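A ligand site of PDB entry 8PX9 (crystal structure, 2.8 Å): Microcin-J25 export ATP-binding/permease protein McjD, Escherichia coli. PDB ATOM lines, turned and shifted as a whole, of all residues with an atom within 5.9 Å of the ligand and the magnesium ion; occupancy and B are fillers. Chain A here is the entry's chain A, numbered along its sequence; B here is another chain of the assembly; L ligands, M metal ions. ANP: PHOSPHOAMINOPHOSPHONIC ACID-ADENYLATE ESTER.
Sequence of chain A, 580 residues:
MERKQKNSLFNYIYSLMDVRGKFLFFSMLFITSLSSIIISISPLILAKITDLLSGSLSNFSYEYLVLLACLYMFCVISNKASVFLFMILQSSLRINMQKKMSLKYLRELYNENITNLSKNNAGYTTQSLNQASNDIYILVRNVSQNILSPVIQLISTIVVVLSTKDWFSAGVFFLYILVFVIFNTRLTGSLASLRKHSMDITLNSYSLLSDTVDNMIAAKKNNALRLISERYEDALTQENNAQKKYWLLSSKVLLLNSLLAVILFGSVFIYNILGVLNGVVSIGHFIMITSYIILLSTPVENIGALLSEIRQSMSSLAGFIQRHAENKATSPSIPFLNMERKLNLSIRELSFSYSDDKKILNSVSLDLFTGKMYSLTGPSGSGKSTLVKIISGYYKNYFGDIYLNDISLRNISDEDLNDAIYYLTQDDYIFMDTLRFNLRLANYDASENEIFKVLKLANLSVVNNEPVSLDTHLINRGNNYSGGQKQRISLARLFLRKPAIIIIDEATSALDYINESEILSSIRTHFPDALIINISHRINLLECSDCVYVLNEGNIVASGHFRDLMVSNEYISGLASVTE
The side-chain hydroxyl (OG) of Ser 482 of chain B is in hydrogen-bond range of an oxygen (O2G) of the ligand.
OG of Ser 380 is in hydrogen-bond range of O2G of the ligand, at 3.1 Å.
The backbone NH (N) of Ser 385 sits at hydrogen-bond distance from an oxygen (O1A) of the ligand (3.4 Å).
N of Lys 384 is in hydrogen-bond range of O1B of the ligand.
The side-chain hydroxyl of Thr 386 sits at hydrogen-bond distance from an oxygen (O1A) of the ligand.
The side-chain amide oxygen (OE1) of Gln 485 of chain B sits at hydrogen-bond distance from an oxygen (O2') of the ligand (3.0 Å).
O of Ser 380 lies within hydrogen-bond range of N3B of the ligand, at 2.8 Å.
O1G of the ligand lies within salt-bridge range of NZ of Lys 384 (2.8 Å).
N6 of the ligand lies within hydrogen-bond range of O of Asn 479 of chain B.
An oxygen (O2G) of the ligand sits at hydrogen-bond distance from the backbone NH (N) of Gly 484 of chain B (2.9 Å).
OE2 of Glu 506 sits close to O1G of the ligand (3.0 Å).
O2' of the ligand lies close to O of Asn 480 of chain B, 3.5 Å away.
The backbone NH of Gly 383 lies within hydrogen-bond range of an oxygen (O1B) of the ligand (2.8 Å).
An oxygen (O1A) of the ligand lies within hydrogen-bond range of the backbone NH (N) of Thr 386 (2.8 Å).
The side-chain amino group (NZ) of Lys 384 lies within hydrogen-bond range of the backbone carbonyl oxygen (O) of Pro 379, at 3.3 Å.
The side-chain amino group of Lys 384 lies within hydrogen-bond range of a ring nitrogen (NE2) of His 537 (2.9 Å).
The backbone NH (N) of Glu 506 sits at hydrogen-bond distance from the backbone carbonyl oxygen (O) of Ile 535 (3.1 Å).
O of Ser 380 lies within hydrogen-bond range of OG of Ser 482 of chain B, 3.3 Å away.
NZ of Lys 384 sits at hydrogen-bond distance from O of Gly 378, at 3.1 Å.
OD2 of Asp 505 lies close to OG of Ser 385 (2.7 Å).
The side-chain hydroxyl (OG1) of Thr 386 sits at hydrogen-bond distance from the side-chain hydroxyl (OH) of Tyr 354 (2.8 Å).
A ring nitrogen (NE2) of His 537 lies within hydrogen-bond range of the backbone carbonyl oxygen (O) of Gly 378, at 3.3 Å.
Merely in contact with the ligand: Tyr 354, Ile 360, Pro 379, Gly 381, Ser 382, His 537, Val 463 of chain B, Tyr 481 of chain B, Gly 483 of chain B and Ala 510 of chain B.
Of the 32 residues printed, 22 come within 4 Å of the ligand.
Asp 505 touches the magnesium ion.
The nearest printed residue that does not touch the magnesium ion is Gly 483 of chain B (4.5 Å).
O3G of the ligand is bound to the magnesium ion (1.9 Å).
The magnesium ion is bound by the side-chain hydroxyl (OG) of Ser 385, 2.0 Å away.
The magnesium ion is bound by OE1 of Gln 426 (2.0 Å).
An oxygen (O2B) of the ligand binds the magnesium ion.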
ATOM      1  N   TYR A 354      10.300  -2.200  -5.942  1.00  0.00           N
ATOM      2  CA  TYR A 354       9.806  -0.887  -6.362  1.00  0.00           C
ATOM      3  C   TYR A 354      10.107  -0.679  -7.853  1.00  0.00           C
ATOM      4  O   TYR A 354       9.246  -0.244  -8.614  1.00  0.00           O
ATOM      5  CB  TYR A 354      10.437   0.215  -5.500  1.00  0.00           C
ATOM      6  CG  TYR A 354       9.783   0.389  -4.148  1.00  0.00           C
ATOM      7  CD1 TYR A 354       8.601   1.119  -4.009  1.00  0.00           C
ATOM      8  CD2 TYR A 354      10.343  -0.154  -3.006  1.00  0.00           C
ATOM      9  CE1 TYR A 354       8.012   1.300  -2.771  1.00  0.00           C
ATOM     10  CE2 TYR A 354       9.761   0.017  -1.752  1.00  0.00           C
ATOM     11  CZ  TYR A 354       8.585   0.745  -1.642  1.00  0.00           C
ATOM     12  OH  TYR A 354       7.988   0.921  -0.416  1.00  0.00           O
ATOM     13  N   SER A 355      11.353  -1.002  -8.267  1.00  0.00           N
ATOM     14  CA  SER A 355      11.829  -1.121  -9.640  1.00  0.00           C
ATOM     15  C   SER A 355      12.370  -2.548  -9.839  1.00  0.00           C
ATOM     16  O   SER A 355      12.871  -3.132  -8.891  1.00  0.00           O
ATOM     17  CB  SER A 355      12.907  -0.086  -9.872  1.00  0.00           C
ATOM     18  OG  SER A 355      14.086  -0.368  -9.089  1.00  0.00           O
ATOM     19  N   ILE A 360      13.270  -5.778  -2.756  1.00  0.00           N
ATOM     20  CA  ILE A 360      13.092  -5.238  -1.414  1.00  0.00           C
ATOM     21  C   ILE A 360      12.643  -6.309  -0.435  1.00  0.00           C
ATOM     22  O   ILE A 360      13.158  -6.378   0.671  1.00  0.00           O
ATOM     23  CB  ILE A 360      12.202  -3.975  -1.450  1.00  0.00           C
ATOM     24  CG1 ILE A 360      12.893  -2.872  -2.279  1.00  0.00           C
ATOM     25  CG2 ILE A 360      11.918  -3.440  -0.048  1.00  0.00           C
ATOM     26  CD1 ILE A 360      14.286  -2.410  -1.790  1.00  0.00           C
ATOM     27  N   GLY A 378      14.551  -4.345  12.362  1.00  0.00           N
ATOM     28  CA  GLY A 378      15.657  -4.612  11.463  1.00  0.00           C
ATOM     29  C   GLY A 378      16.310  -3.307  11.038  1.00  0.00           C
ATOM     30  O   GLY A 378      15.851  -2.218  11.419  1.00  0.00           O
ATOM     31  N   PRO A 379      17.352  -3.377  10.193  1.00  0.00           N
ATOM     32  CA  PRO A 379      17.999  -2.136   9.735  1.00  0.00           C
ATOM     33  C   PRO A 379      17.100  -1.289   8.826  1.00  0.00           C
ATOM     34  O   PRO A 379      15.951  -1.679   8.559  1.00  0.00           O
ATOM     35  CB  PRO A 379      19.273  -2.634   9.036  1.00  0.00           C
ATOM     36  CG  PRO A 379      19.423  -4.091   9.465  1.00  0.00           C
ATOM     37  CD  PRO A 379      18.005  -4.583   9.654  1.00  0.00           C
ATOM     38  N   SER A 380      17.570  -0.115   8.365  1.00  0.00           N
ATOM     39  CA  SER A 380      16.746   0.797   7.568  1.00  0.00           C
ATOM     40  C   SER A 380      16.436   0.290   6.154  1.00  0.00           C
ATOM     41  O   SER A 380      15.414   0.673   5.576  1.00  0.00           O
ATOM     42  CB  SER A 380      17.307   2.191   7.485  1.00  0.00           C
ATOM     43  OG  SER A 380      17.291   2.852   8.731  1.00  0.00           O
ATOM     44  N   GLY A 381      17.311  -0.562   5.596  1.00  0.00           N
ATOM     45  CA  GLY A 381      17.123  -1.076   4.256  1.00  0.00           C
ATOM     46  C   GLY A 381      16.364  -2.400   4.174  1.00  0.00           C
ATOM     47  O   GLY A 381      16.115  -2.886   3.066  1.00  0.00           O
ATOM     48  N   SER A 382      16.000  -2.988   5.322  1.00  0.00           N
ATOM     49  CA  SER A 382      15.320  -4.272   5.386  1.00  0.00           C
ATOM     50  C   SER A 382      13.921  -4.263   4.767  1.00  0.00           C
ATOM     51  O   SER A 382      13.552  -5.212   4.076  1.00  0.00           O
ATOM     52  CB  SER A 382      15.269  -4.793   6.819  1.00  0.00           C
ATOM     53  OG  SER A 382      14.609  -3.873   7.673  1.00  0.00           O
ATOM     54  N   GLY A 383      13.164  -3.185   4.998  1.00  0.00           N
ATOM     55  CA  GLY A 383      11.843  -3.040   4.393  1.00  0.00           C
ATOM     56  C   GLY A 383      10.663  -3.359   5.297  1.00  0.00           C
ATOM     57  O   GLY A 383       9.746  -4.093   4.926  1.00  0.00           O
ATOM     58  N   LYS A 384      10.663  -2.770   6.508  1.00  0.00           N
ATOM     59  CA  LYS A 384       9.573  -2.913   7.455  1.00  0.00           C
ATOM     60  C   LYS A 384       8.372  -2.113   6.948  1.00  0.00           C
ATOM     61  O   LYS A 384       7.277  -2.648   6.860  1.00  0.00           O
ATOM     62  CB  LYS A 384       9.965  -2.472   8.868  1.00  0.00           C
ATOM     63  CG  LYS A 384      10.993  -3.326   9.576  1.00  0.00           C
ATOM     64  CD  LYS A 384      12.333  -2.635   9.721  1.00  0.00           C
ATOM     65  CE  LYS A 384      12.298  -1.427  10.649  1.00  0.00           C
ATOM     66  NZ  LYS A 384      13.423  -0.525  10.395  1.00  0.00           N
ATOM     67  N   SER A 385       8.606  -0.835   6.572  1.00  0.00           N
ATOM     68  CA  SER A 385       7.583   0.067   6.062  1.00  0.00           C
ATOM     69  C   SER A 385       6.979  -0.430   4.743  1.00  0.00           C
ATOM     70  O   SER A 385       5.781  -0.350   4.577  1.00  0.00           O
ATOM     71  CB  SER A 385       8.107   1.467   5.913  1.00  0.00           C
ATOM     72  OG  SER A 385       8.514   1.973   7.169  1.00  0.00           O
ATOM     73  N   THR A 386       7.818  -0.949   3.818  1.00  0.00           N
ATOM     74  CA  THR A 386       7.345  -1.496   2.558  1.00  0.00           C
ATOM     75  C   THR A 386       6.347  -2.638   2.779  1.00  0.00           C
ATOM     76  O   THR A 386       5.229  -2.600   2.278  1.00  0.00           O
ATOM     77  CB  THR A 386       8.551  -1.872   1.663  1.00  0.00           C
ATOM     78  OG1 THR A 386       9.345  -0.731   1.352  1.00  0.00           O
ATOM     79  CG2 THR A 386       8.198  -2.738   0.465  1.00  0.00           C
ATOM     80  N   LEU A 387       6.733  -3.616   3.624  1.00  0.00           N
ATOM     81  CA  LEU A 387       5.937  -4.785   3.982  1.00  0.00           C
ATOM     82  C   LEU A 387       4.580  -4.376   4.522  1.00  0.00           C
ATOM     83  O   LEU A 387       3.560  -4.902   4.093  1.00  0.00           O
ATOM     84  CB  LEU A 387       6.716  -5.599   5.017  1.00  0.00           C
ATOM     85  CG  LEU A 387       6.174  -6.991   5.377  1.00  0.00           C
ATOM     86  CD1 LEU A 387       7.311  -7.982   5.584  1.00  0.00           C
ATOM     87  CD2 LEU A 387       5.364  -6.946   6.657  1.00  0.00           C
ATOM     88  N   LYS A 389       3.153  -1.367   4.167  1.00  0.00           N
ATOM     89  CA  LYS A 389       2.462  -0.587   3.133  1.00  0.00           C
ATOM     90  C   LYS A 389       1.707  -1.520   2.189  1.00  0.00           C
ATOM     91  O   LYS A 389       0.603  -1.183   1.786  1.00  0.00           O
ATOM     92  CB  LYS A 389       3.448   0.303   2.355  1.00  0.00           C
ATOM     93  CG  LYS A 389       3.858   1.583   3.062  1.00  0.00           C
ATOM     94  CD  LYS A 389       4.976   2.283   2.326  1.00  0.00           C
ATOM     95  CE  LYS A 389       5.833   3.191   3.170  1.00  0.00           C
ATOM     96  NZ  LYS A 389       5.092   4.377   3.641  1.00  0.00           N
ATOM     97  N   TYR A 395       0.735  -0.528  -2.439  1.00  0.00           N
ATOM     98  CA  TYR A 395       1.273  -1.099  -3.672  1.00  0.00           C
ATOM     99  C   TYR A 395       0.605  -2.468  -3.909  1.00  0.00           C
ATOM    100  O   TYR A 395       0.472  -3.277  -2.983  1.00  0.00           O
ATOM    101  CB  TYR A 395       2.798  -1.222  -3.574  1.00  0.00           C
ATOM    102  CG  TYR A 395       3.487   0.020  -3.021  1.00  0.00           C
ATOM    103  CD1 TYR A 395       3.639   1.171  -3.789  1.00  0.00           C
ATOM    104  CD2 TYR A 395       3.938   0.045  -1.708  1.00  0.00           C
ATOM    105  CE1 TYR A 395       4.245   2.308  -3.268  1.00  0.00           C
ATOM    106  CE2 TYR A 395       4.527   1.185  -1.176  1.00  0.00           C
ATOM    107  CZ  TYR A 395       4.676   2.314  -1.943  1.00  0.00           C
ATOM    108  OH  TYR A 395       5.288   3.428  -1.425  1.00  0.00           O
ATOM    109  N   GLN A 426       4.897   6.499   9.300  1.00  0.00           N
ATOM    110  CA  GLN A 426       6.151   6.935   9.878  1.00  0.00           C
ATOM    111  C   GLN A 426       6.226   8.464   9.904  1.00  0.00           C
ATOM    112  O   GLN A 426       6.618   9.052  10.927  1.00  0.00           O
ATOM    113  CB  GLN A 426       7.329   6.332   9.104  1.00  0.00           C
ATOM    114  CG  GLN A 426       8.515   5.952   9.990  1.00  0.00           C
ATOM    115  CD  GLN A 426       9.608   5.221   9.247  1.00  0.00           C
ATOM    116  OE1 GLN A 426       9.341   4.328   8.452  1.00  0.00           O
ATOM    117  NE2 GLN A 426      10.871   5.607   9.407  1.00  0.00           N
ATOM    118  N   ASP A 505       3.873   2.238  12.764  1.00  0.00           N
ATOM    119  CA  ASP A 505       5.188   2.312  12.130  1.00  0.00           C
ATOM    120  C   ASP A 505       5.940   3.519  12.683  1.00  0.00           C
ATOM    121  O   ASP A 505       5.856   4.611  12.130  1.00  0.00           O
ATOM    122  CB  ASP A 505       5.027   2.393  10.602  1.00  0.00           C
ATOM    123  CG  ASP A 505       6.301   2.329   9.774  1.00  0.00           C
ATOM    124  OD1 ASP A 505       7.376   2.034  10.338  1.00  0.00           O
ATOM    125  OD2 ASP A 505       6.220   2.550   8.546  1.00  0.00           O
ATOM    126  N   GLU A 506       6.679   3.316  13.794  1.00  0.00           N
ATOM    127  CA  GLU A 506       7.472   4.350  14.491  1.00  0.00           C
ATOM    128  C   GLU A 506       6.669   5.622  14.766  1.00  0.00           C
ATOM    129  O   GLU A 506       7.257   6.699  14.865  1.00  0.00           O
ATOM    130  CB  GLU A 506       8.803   4.598  13.772  1.00  0.00           C
ATOM    131  CG  GLU A 506       9.620   3.327  13.541  1.00  0.00           C
ATOM    132  CD  GLU A 506      11.023   3.529  12.962  1.00  0.00           C
ATOM    133  OE1 GLU A 506      11.616   4.628  13.146  1.00  0.00           O
ATOM    134  OE2 GLU A 506      11.621   2.547  12.425  1.00  0.00           O
ATOM    135  N   ILE A 535       6.341  -1.382  14.614  1.00  0.00           N
ATOM    136  CA  ILE A 535       7.672  -1.238  14.049  1.00  0.00           C
ATOM    137  C   ILE A 535       8.440  -0.290  14.971  1.00  0.00           C
ATOM    138  O   ILE A 535       7.988   0.833  15.193  1.00  0.00           O
ATOM    139  CB  ILE A 535       7.655  -0.779  12.577  1.00  0.00           C
ATOM    140  CG1 ILE A 535       6.927  -1.790  11.663  1.00  0.00           C
ATOM    141  CG2 ILE A 535       9.061  -0.501  12.063  1.00  0.00           C
ATOM    142  CD1 ILE A 535       5.544  -1.388  11.281  1.00  0.00           C
ATOM    143  N   HIS A 537      12.758   0.467  16.850  1.00  0.00           N
ATOM    144  CA  HIS A 537      14.175   0.167  17.075  1.00  0.00           C
ATOM    145  C   HIS A 537      14.519   0.179  18.593  1.00  0.00           C
ATOM    146  O   HIS A 537      15.695   0.090  18.926  1.00  0.00           O
ATOM    147  CB  HIS A 537      15.055   1.202  16.354  1.00  0.00           C
ATOM    148  CG  HIS A 537      14.950   1.147  14.860  1.00  0.00           C
ATOM    149  ND1 HIS A 537      14.816   2.285  14.084  1.00  0.00           N
ATOM    150  CD2 HIS A 537      14.925   0.105  14.003  1.00  0.00           C
ATOM    151  CE1 HIS A 537      14.779   1.911  12.825  1.00  0.00           C
ATOM    152  NE2 HIS A 537      14.802   0.592  12.746  1.00  0.00           N
ATOM    153  N   LEU A 551      13.527  -8.629  10.552  1.00  0.00           N
ATOM    154  CA  LEU A 551      13.612  -8.548   9.105  1.00  0.00           C
ATOM    155  C   LEU A 551      14.997  -8.014   8.745  1.00  0.00           C
ATOM    156  O   LEU A 551      15.401  -6.959   9.242  1.00  0.00           O
ATOM    157  CB  LEU A 551      12.517  -7.609   8.601  1.00  0.00           C
ATOM    158  CG  LEU A 551      12.349  -7.485   7.087  1.00  0.00           C
ATOM    159  CD1 LEU A 551      11.779  -8.728   6.477  1.00  0.00           C
ATOM    160  CD2 LEU A 551      11.423  -6.343   6.778  1.00  0.00           C
ATOM    161  N   VAL B 463      23.570   0.651   0.094  1.00  0.00           N
ATOM    162  CA  VAL B 463      22.156   0.438   0.412  1.00  0.00           C
ATOM    163  C   VAL B 463      21.683  -0.771  -0.386  1.00  0.00           C
ATOM    164  O   VAL B 463      21.918  -0.817  -1.591  1.00  0.00           O
ATOM    165  CB  VAL B 463      21.292   1.679   0.079  1.00  0.00           C
ATOM    166  CG1 VAL B 463      19.829   1.510   0.482  1.00  0.00           C
ATOM    167  CG2 VAL B 463      21.838   2.962   0.697  1.00  0.00           C
ATOM    168  N   ASN B 464      20.978  -1.725   0.272  1.00  0.00           N
ATOM    169  CA  ASN B 464      20.380  -2.910  -0.343  1.00  0.00           C
ATOM    170  C   ASN B 464      21.464  -3.817  -0.969  1.00  0.00           C
ATOM    171  O   ASN B 464      21.237  -4.398  -2.030  1.00  0.00           O
ATOM    172  CB  ASN B 464      19.262  -2.468  -1.312  1.00  0.00           C
ATOM    173  CG  ASN B 464      18.168  -3.487  -1.561  1.00  0.00           C
ATOM    174  OD1 ASN B 464      17.662  -4.092  -0.616  1.00  0.00           O
ATOM    175  ND2 ASN B 464      17.760  -3.677  -2.812  1.00  0.00           N
ATOM    176  N   ILE B 475      12.666  11.536  -5.029  1.00  0.00           N
ATOM    177  CA  ILE B 475      11.338  12.053  -5.349  1.00  0.00           C
ATOM    178  C   ILE B 475      10.887  13.093  -4.305  1.00  0.00           C
ATOM    179  O   ILE B 475      11.654  13.472  -3.440  1.00  0.00           O
ATOM    180  CB  ILE B 475      10.337  10.887  -5.574  1.00  0.00           C
ATOM    181  CG1 ILE B 475       9.965  10.151  -4.295  1.00  0.00           C
ATOM    182  CG2 ILE B 475      10.834   9.937  -6.665  1.00  0.00           C
ATOM    183  CD1 ILE B 475       8.696   9.321  -4.416  1.00  0.00           C
ATOM    184  N   ASN B 479      10.605  10.535  -0.452  1.00  0.00           N
ATOM    185  CA  ASN B 479       9.874   9.345  -0.013  1.00  0.00           C
ATOM    186  C   ASN B 479      10.205   8.094  -0.858  1.00  0.00           C
ATOM    187  O   ASN B 479       9.478   7.106  -0.779  1.00  0.00           O
ATOM    188  CB  ASN B 479       8.350   9.534   0.074  1.00  0.00           C
ATOM    189  CG  ASN B 479       7.874  10.840   0.708  1.00  0.00           C
ATOM    190  OD1 ASN B 479       7.391  11.703  -0.006  1.00  0.00           O
ATOM    191  ND2 ASN B 479       7.893  10.959   2.032  1.00  0.00           N
ATOM    192  N   ASN B 480      11.285   8.107  -1.662  1.00  0.00           N
ATOM    193  CA  ASN B 480      11.855   6.899  -2.262  1.00  0.00           C
ATOM    194  C   ASN B 480      12.991   6.293  -1.417  1.00  0.00           C
ATOM    195  O   ASN B 480      13.603   5.325  -1.853  1.00  0.00           O
ATOM    196  CB  ASN B 480      12.228   7.117  -3.732  1.00  0.00           C
ATOM    197  CG  ASN B 480      13.296   8.173  -3.948  1.00  0.00           C
ATOM    198  OD1 ASN B 480      13.242   9.237  -3.339  1.00  0.00           O
ATOM    199  ND2 ASN B 480      14.241   7.901  -4.822  1.00  0.00           N
ATOM    200  N   TYR B 481      13.254   6.894  -0.238  1.00  0.00           N
ATOM    201  CA  TYR B 481      14.190   6.475   0.794  1.00  0.00           C
ATOM    202  C   TYR B 481      13.422   6.322   2.104  1.00  0.00           C
ATOM    203  O   TYR B 481      12.463   7.079   2.339  1.00  0.00           O
ATOM    204  CB  TYR B 481      15.276   7.573   0.903  1.00  0.00           C
ATOM    205  CG  TYR B 481      16.560   7.352   0.119  1.00  0.00           C
ATOM    206  CD1 TYR B 481      16.587   6.691  -1.107  1.00  0.00           C
ATOM    207  CD2 TYR B 481      17.762   7.866   0.604  1.00  0.00           C
ATOM    208  CE1 TYR B 481      17.778   6.480  -1.792  1.00  0.00           C
ATOM    209  CE2 TYR B 481      18.968   7.685  -0.083  1.00  0.00           C
ATOM    210  CZ  TYR B 481      18.966   6.993  -1.289  1.00  0.00           C
ATOM    211  OH  TYR B 481      20.105   6.792  -2.006  1.00  0.00           O
ATOM    212  N   SER B 482      13.883   5.390   2.963  1.00  0.00           N
ATOM    213  CA  SER B 482      13.257   5.127   4.269  1.00  0.00           C
ATOM    214  C   SER B 482      13.468   6.296   5.231  1.00  0.00           C
ATOM    215  O   SER B 482      14.337   7.142   4.993  1.00  0.00           O
ATOM    216  CB  SER B 482      13.735   3.836   4.857  1.00  0.00           C
ATOM    217  OG  SER B 482      15.027   3.986   5.405  1.00  0.00           O
ATOM    218  N   GLY B 483      12.675   6.327   6.321  1.00  0.00           N
ATOM    219  CA  GLY B 483      12.735   7.429   7.281  1.00  0.00           C
ATOM    220  C   GLY B 483      14.132   7.622   7.878  1.00  0.00           C
ATOM    221  O   GLY B 483      14.567   8.761   7.998  1.00  0.00           O
ATOM    222  N   GLY B 484      14.811   6.504   8.195  1.00  0.00           N
ATOM    223  CA  GLY B 484      16.184   6.521   8.680  1.00  0.00           C
ATOM    224  C   GLY B 484      17.183   6.948   7.612  1.00  0.00           C
ATOM    225  O   GLY B 484      18.125   7.671   7.928  1.00  0.00           O
ATOM    226  N   GLN B 485      16.968   6.512   6.366  1.00  0.00           N
ATOM    227  CA  GLN B 485      17.803   6.893   5.227  1.00  0.00           C
ATOM    228  C   GLN B 485      17.722   8.384   4.908  1.00  0.00           C
ATOM    229  O   GLN B 485      18.693   8.951   4.403  1.00  0.00           O
ATOM    230  CB  GLN B 485      17.446   6.052   3.995  1.00  0.00           C
ATOM    231  CG  GLN B 485      17.954   4.628   4.062  1.00  0.00           C
ATOM    232  CD  GLN B 485      17.926   3.997   2.692  1.00  0.00           C
ATOM    233  OE1 GLN B 485      17.029   3.234   2.345  1.00  0.00           O
ATOM    234  NE2 GLN B 485      18.925   4.333   1.896  1.00  0.00           N
ATOM    235  N   ALA B 510      14.883   7.516  13.876  1.00  0.00           N
ATOM    236  CA  ALA B 510      14.553   6.416  12.971  1.00  0.00           C
ATOM    237  C   ALA B 510      15.755   5.545  12.582  1.00  0.00           C
ATOM    238  O   ALA B 510      15.613   4.771  11.645  1.00  0.00           O
ATOM    239  CB  ALA B 510      13.884   6.981  11.732  1.00  0.00           C
HETATM  240  PG  ANP L   1      13.269   2.617   8.480  1.00  0.00           P
HETATM  241  O1G ANP L   1      13.254   2.247   9.930  1.00  0.00           O
HETATM  242  O2G ANP L   1      14.312   3.640   8.108  1.00  0.00           O
HETATM  243  O3G ANP L   1      11.963   3.269   8.262  1.00  0.00           O
HETATM  244  PB  ANP L   1      12.383   0.455   6.711  1.00  0.00           P
HETATM  245  O1B ANP L   1      12.905  -0.951   6.656  1.00  0.00           O
HETATM  246  O2B ANP L   1      10.970   0.729   7.152  1.00  0.00           O
HETATM  247  N3B ANP L   1      13.467   1.423   7.407  1.00  0.00           N
HETATM  248  PA  ANP L   1      11.481   1.037   3.918  1.00  0.00           P
HETATM  249  O1A ANP L   1      10.461  -0.062   3.863  1.00  0.00           O
HETATM  250  O2A ANP L   1      10.975   2.432   4.045  1.00  0.00           O
HETATM  251  O3A ANP L   1      12.489   0.856   5.148  1.00  0.00           O
HETATM  252  O5' ANP L   1      12.470   0.911   2.669  1.00  0.00           O
HETATM  253  C5' ANP L   1      13.143  -0.325   2.401  1.00  0.00           C
HETATM  254  C4' ANP L   1      13.988  -0.214   1.156  1.00  0.00           C
HETATM  255  O4' ANP L   1      13.117   0.179   0.065  1.00  0.00           O
HETATM  256  C3' ANP L   1      15.138   0.809   1.156  1.00  0.00           C
HETATM  257  O3' ANP L   1      16.221   0.316   0.365  1.00  0.00           O
HETATM  258  C2' ANP L   1      14.494   2.046   0.517  1.00  0.00           C
HETATM  259  O2' ANP L   1      15.417   2.870  -0.169  1.00  0.00           O
HETATM  260  C1' ANP L   1      13.546   1.402  -0.484  1.00  0.00           C
HETATM  261  N9  ANP L   1      12.354   2.232  -0.780  1.00  0.00           N
HETATM  262  C8  ANP L   1      11.393   2.710   0.106  1.00  0.00           C
HETATM  263  N7  ANP L   1      10.456   3.416  -0.480  1.00  0.00           N
HETATM  264  C5  ANP L   1      10.817   3.408  -1.823  1.00  0.00           C
HETATM  265  C6  ANP L   1      10.212   3.957  -2.965  1.00  0.00           C
HETATM  266  N6  ANP L   1       9.101   4.691  -2.906  1.00  0.00           N
HETATM  267  N1  ANP L   1      10.836   3.770  -4.160  1.00  0.00           N
HETATM  268  C2  ANP L   1      11.971   3.030  -4.196  1.00  0.00           C
HETATM  269  N3  ANP L   1      12.615   2.459  -3.184  1.00  0.00           N
HETATM  270  C4  ANP L   1      11.970   2.674  -2.013  1.00  0.00           C
HETATM  271 MG    MG M   1      10.269   2.745   7.671  1.00  0.00          MG
